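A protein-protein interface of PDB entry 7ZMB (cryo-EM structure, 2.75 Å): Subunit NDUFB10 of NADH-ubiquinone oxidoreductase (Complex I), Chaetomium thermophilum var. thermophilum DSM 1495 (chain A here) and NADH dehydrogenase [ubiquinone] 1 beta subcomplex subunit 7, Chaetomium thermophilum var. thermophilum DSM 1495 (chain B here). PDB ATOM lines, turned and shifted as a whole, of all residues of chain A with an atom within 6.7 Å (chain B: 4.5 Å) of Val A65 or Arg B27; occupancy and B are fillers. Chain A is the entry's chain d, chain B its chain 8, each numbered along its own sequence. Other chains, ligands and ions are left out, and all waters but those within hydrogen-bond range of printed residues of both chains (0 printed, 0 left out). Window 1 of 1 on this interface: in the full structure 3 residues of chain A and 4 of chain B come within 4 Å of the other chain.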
ATOM      1  N   TYR A  60      29.500  -4.669  13.550  1.00  0.00           N
ATOM      2  CA  TYR A  60      29.715  -4.153  14.894  1.00  0.00           C
ATOM      3  C   TYR A  60      29.860  -2.641  14.905  1.00  0.00           C
ATOM      4  O   TYR A  60      29.391  -1.971  15.833  1.00  0.00           O
ATOM      5  CB  TYR A  60      30.946  -4.786  15.528  1.00  0.00           C
ATOM      6  CG  TYR A  60      31.116  -4.285  16.932  1.00  0.00           C
ATOM      7  CD1 TYR A  60      30.205  -4.631  17.908  1.00  0.00           C
ATOM      8  CD2 TYR A  60      32.147  -3.418  17.267  1.00  0.00           C
ATOM      9  CE1 TYR A  60      30.330  -4.166  19.184  1.00  0.00           C
ATOM     10  CE2 TYR A  60      32.280  -2.949  18.550  1.00  0.00           C
ATOM     11  CZ  TYR A  60      31.362  -3.329  19.504  1.00  0.00           C
ATOM     12  OH  TYR A  60      31.465  -2.883  20.795  1.00  0.00           O
ATOM     13  N   GLU A  63      26.208  -0.987  13.656  1.00  0.00           N
ATOM     14  CA  GLU A  63      25.073  -1.015  14.564  1.00  0.00           C
ATOM     15  C   GLU A  63      25.382  -0.403  15.920  1.00  0.00           C
ATOM     16  O   GLU A  63      24.635   0.459  16.392  1.00  0.00           O
ATOM     17  CB  GLU A  63      24.572  -2.455  14.737  1.00  0.00           C
ATOM     18  CG  GLU A  63      23.925  -3.026  13.485  1.00  0.00           C
ATOM     19  CD  GLU A  63      23.127  -1.991  12.709  1.00  0.00           C
ATOM     20  OE1 GLU A  63      22.263  -1.316  13.309  1.00  0.00           O
ATOM     21  OE2 GLU A  63      23.369  -1.849  11.493  1.00  0.00           O
ATOM     22  N   GLY A  64      26.459  -0.828  16.568  1.00  0.00           N
ATOM     23  CA  GLY A  64      26.858  -0.204  17.810  1.00  0.00           C
ATOM     24  C   GLY A  64      26.018  -0.623  18.996  1.00  0.00           C
ATOM     25  O   GLY A  64      26.151  -1.743  19.500  1.00  0.00           O
ATOM     26  N   VAL A  65      25.155   0.284  19.460  1.00  0.00           N
ATOM     27  CA  VAL A  65      24.276  -0.025  20.585  1.00  0.00           C
ATOM     28  C   VAL A  65      23.398  -1.226  20.263  1.00  0.00           C
ATOM     29  O   VAL A  65      23.303  -2.176  21.049  1.00  0.00           O
ATOM     30  CB  VAL A  65      23.437   1.209  20.955  1.00  0.00           C
ATOM     31  CG1 VAL A  65      22.238   0.808  21.770  1.00  0.00           C
ATOM     32  CG2 VAL A  65      24.278   2.167  21.756  1.00  0.00           C
ATOM     33  N   ASN A  66      22.745  -1.206  19.107  1.00  0.00           N
ATOM     34  CA  ASN A  66      21.908  -2.329  18.693  1.00  0.00           C
ATOM     35  C   ASN A  66      22.667  -3.334  17.826  1.00  0.00           C
ATOM     36  O   ASN A  66      22.192  -3.786  16.787  1.00  0.00           O
ATOM     37  CB  ASN A  66      20.657  -1.795  17.997  1.00  0.00           C
ATOM     38  CG  ASN A  66      20.945  -1.147  16.649  1.00  0.00           C
ATOM     39  OD1 ASN A  66      22.080  -1.123  16.175  1.00  0.00           O
ATOM     40  ND2 ASN A  66      19.903  -0.611  16.025  1.00  0.00           N
ATOM     41  N   HIS A  67      23.841  -3.759  18.300  1.00  0.00           N
ATOM     42  CA  HIS A  67      24.662  -4.761  17.568  1.00  0.00           C
ATOM     43  C   HIS A  67      24.345  -6.165  18.077  1.00  0.00           C
ATOM     44  O   HIS A  67      24.577  -7.126  17.331  1.00  0.00           O
ATOM     45  CB  HIS A  67      26.153  -4.451  17.732  1.00  0.00           C
ATOM     46  CG  HIS A  67      26.776  -4.995  18.974  1.00  0.00           C
ATOM     47  ND1 HIS A  67      27.475  -6.185  18.990  1.00  0.00           N
ATOM     48  CD2 HIS A  67      26.827  -4.516  20.234  1.00  0.00           C
ATOM     49  CE1 HIS A  67      27.925  -6.413  20.205  1.00  0.00           C
ATOM     50  NE2 HIS A  67      27.544  -5.403  20.985  1.00  0.00           N
ATOM     51  N   LEU A  68      23.829  -6.266  19.301  1.00  0.00           N
ATOM     52  CA  LEU A  68      23.554  -7.573  19.867  1.00  0.00           C
ATOM     53  C   LEU A  68      22.269  -8.179  19.335  1.00  0.00           C
ATOM     54  O   LEU A  68      21.958  -9.325  19.674  1.00  0.00           O
ATOM     55  CB  LEU A  68      23.510  -7.474  21.389  1.00  0.00           C
ATOM     56  CG  LEU A  68      24.871  -7.182  22.015  1.00  0.00           C
ATOM     57  CD1 LEU A  68      24.734  -6.773  23.468  1.00  0.00           C
ATOM     58  CD2 LEU A  68      25.764  -8.403  21.890  1.00  0.00           C
ATOM     59  N   GLU A  69      21.523  -7.453  18.499  1.00  0.00           N
ATOM     60  CA  GLU A  69      20.259  -7.969  17.995  1.00  0.00           C
ATOM     61  C   GLU A  69      20.060  -7.742  16.502  1.00  0.00           C
ATOM     62  O   GLU A  69      18.929  -7.887  16.020  1.00  0.00           O
ATOM     63  CB  GLU A  69      19.088  -7.350  18.769  1.00  0.00           C
ATOM     64  CG  GLU A  69      18.858  -5.877  18.491  1.00  0.00           C
ATOM     65  CD  GLU A  69      17.442  -5.441  18.818  1.00  0.00           C
ATOM     66  OE1 GLU A  69      16.559  -6.319  18.922  1.00  0.00           O
ATOM     67  OE2 GLU A  69      17.212  -4.224  18.973  1.00  0.00           O
ATOM     68  N   MET B  17      11.413   2.377  18.464  1.00  0.00           N
ATOM     69  CA  MET B  17      12.344   2.900  19.457  1.00  0.00           C
ATOM     70  C   MET B  17      13.758   2.375  19.243  1.00  0.00           C
ATOM     71  O   MET B  17      14.726   3.063  19.584  1.00  0.00           O
ATOM     72  CB  MET B  17      11.818   2.574  20.860  1.00  0.00           C
ATOM     73  CG  MET B  17      12.630   3.098  22.033  1.00  0.00           C
ATOM     74  SD  MET B  17      14.033   2.058  22.455  1.00  0.00           S
ATOM     75  CE  MET B  17      13.184   0.662  23.188  1.00  0.00           C
ATOM     76  N   VAL B  22      18.883   4.429  21.100  1.00  0.00           N
ATOM     77  CA  VAL B  22      19.011   4.957  22.454  1.00  0.00           C
ATOM     78  C   VAL B  22      19.759   3.934  23.304  1.00  0.00           C
ATOM     79  O   VAL B  22      19.758   2.741  22.971  1.00  0.00           O
ATOM     80  CB  VAL B  22      17.634   5.295  23.047  1.00  0.00           C
ATOM     81  CG1 VAL B  22      16.891   6.246  22.127  1.00  0.00           C
ATOM     82  CG2 VAL B  22      16.834   4.035  23.276  1.00  0.00           C
ATOM     83  N   PRO B  23      20.413   4.345  24.391  1.00  0.00           N
ATOM     84  CA  PRO B  23      21.225   3.401  25.169  1.00  0.00           C
ATOM     85  C   PRO B  23      20.386   2.293  25.791  1.00  0.00           C
ATOM     86  O   PRO B  23      19.177   2.425  25.992  1.00  0.00           O
ATOM     87  CB  PRO B  23      21.863   4.284  26.247  1.00  0.00           C
ATOM     88  CG  PRO B  23      21.831   5.658  25.677  1.00  0.00           C
ATOM     89  CD  PRO B  23      20.576   5.729  24.868  1.00  0.00           C
ATOM     90  N   LEU B  24      21.062   1.180  26.093  1.00  0.00           N
ATOM     91  CA  LEU B  24      20.372   0.016  26.643  1.00  0.00           C
ATOM     92  C   LEU B  24      19.732   0.330  27.987  1.00  0.00           C
ATOM     93  O   LEU B  24      18.601  -0.090  28.259  1.00  0.00           O
ATOM     94  CB  LEU B  24      21.338  -1.161  26.794  1.00  0.00           C
ATOM     95  CG  LEU B  24      21.653  -2.051  25.591  1.00  0.00           C
ATOM     96  CD1 LEU B  24      20.389  -2.700  25.044  1.00  0.00           C
ATOM     97  CD2 LEU B  24      22.403  -1.304  24.512  1.00  0.00           C
ATOM     98  N   ALA B  25      20.440   1.064  28.847  1.00  0.00           N
ATOM     99  CA  ALA B  25      19.930   1.355  30.181  1.00  0.00           C
ATOM    100  C   ALA B  25      18.709   2.261  30.164  1.00  0.00           C
ATOM    101  O   ALA B  25      18.057   2.410  31.204  1.00  0.00           O
ATOM    102  CB  ALA B  25      21.028   1.986  31.035  1.00  0.00           C
ATOM    103  N   TYR B  26      18.385   2.868  29.024  1.00  0.00           N
ATOM    104  CA  TYR B  26      17.253   3.777  28.911  1.00  0.00           C
ATOM    105  C   TYR B  26      16.221   3.266  27.912  1.00  0.00           C
ATOM    106  O   TYR B  26      15.454   4.048  27.347  1.00  0.00           O
ATOM    107  CB  TYR B  26      17.731   5.177  28.529  1.00  0.00           C
ATOM    108  CG  TYR B  26      18.787   5.720  29.463  1.00  0.00           C
ATOM    109  CD1 TYR B  26      18.692   5.529  30.833  1.00  0.00           C
ATOM    110  CD2 TYR B  26      19.883   6.413  28.973  1.00  0.00           C
ATOM    111  CE1 TYR B  26      19.654   6.018  31.691  1.00  0.00           C
ATOM    112  CE2 TYR B  26      20.852   6.906  29.825  1.00  0.00           C
ATOM    113  CZ  TYR B  26      20.732   6.706  31.181  1.00  0.00           C
ATOM    114  OH  TYR B  26      21.694   7.195  32.033  1.00  0.00           O
ATOM    115  N   ARG B  27      16.191   1.955  27.684  1.00  0.00           N
ATOM    116  CA  ARG B  27      15.170   1.336  26.848  1.00  0.00           C
ATOM    117  C   ARG B  27      13.829   1.198  27.552  1.00  0.00           C
ATOM    118  O   ARG B  27      12.938   0.527  27.021  1.00  0.00           O
ATOM    119  CB  ARG B  27      15.630  -0.045  26.373  1.00  0.00           C
ATOM    120  CG  ARG B  27      16.889  -0.060  25.530  1.00  0.00           C
ATOM    121  CD  ARG B  27      16.625   0.586  24.190  1.00  0.00           C
ATOM    122  NE  ARG B  27      17.797   0.613  23.326  1.00  0.00           N
ATOM    123  CZ  ARG B  27      18.104  -0.356  22.470  1.00  0.00           C
ATOM    124  NH1 ARG B  27      17.323  -1.421  22.368  1.00  0.00           N
ATOM    125  NH2 ARG B  27      19.186  -0.261  21.713  1.00  0.00           N
ATOM    126  N   ASP B  28      13.661   1.810  28.722  1.00  0.00           N
ATOM    127  CA  ASP B  28      12.439   1.645  29.488  1.00  0.00           C
ATOM    128  C   ASP B  28      11.252   2.272  28.759  1.00  0.00           C
ATOM    129  O   ASP B  28      11.397   2.989  27.765  1.00  0.00           O
ATOM    130  CB  ASP B  28      12.592   2.258  30.881  1.00  0.00           C
ATOM    131  CG  ASP B  28      12.919   3.740  30.837  1.00  0.00           C
ATOM    132  OD1 ASP B  28      13.114   4.284  29.731  1.00  0.00           O
ATOM    133  OD2 ASP B  28      12.976   4.364  31.918  1.00  0.00           O
ATOM    134  N   SER B  29      10.057   1.993  29.279  1.00  0.00           N
ATOM    135  CA  SER B  29       8.832   2.538  28.710  1.00  0.00           C
ATOM    136  C   SER B  29       8.718   4.045  28.892  1.00  0.00           C
ATOM    137  O   SER B  29       7.841   4.662  28.276  1.00  0.00           O
ATOM    138  CB  SER B  29       7.619   1.849  29.332  1.00  0.00           C
ATOM    139  OG  SER B  29       7.483   2.194  30.699  1.00  0.00           O
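NE of Arg B27 is in hydrogen-bond range of O of Val B22 (2.9 Å).
Val B22 touches Val A65 (O to CG1, 3.4 Å).
CG1 of Val A65 touches CD2 of Leu B24, at 3.5 Å.
CG1 of Val A65 touches NH2 of Arg B27, at 3.2 Å.
Gly A64 touches none of the printed residues of chain B.
Of the printed residues of chain A, Val B22 touches Val A65.
Printed residues of chain A within 4 Å of Leu B24: Val A65.
Of the printed residues of chain A, Arg B27 touches Val A65.
The nearest residue of chain B that does not touch Val A65 is Pro B23 (4.4 Å).
Of the 9 printed residues of chain B, 3 touch a printed residue of chain A.
Printed residues of chain B that touch a printed residue of chain A: Val B22, Leu B24 and Arg B27.
Among the printed residues, 3 pairs touch across the chains.
Among the printed residues, no Asp or Glu carboxylate lies within 4 Å of a Lys or Arg side-chain nitrogen of the other chain.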
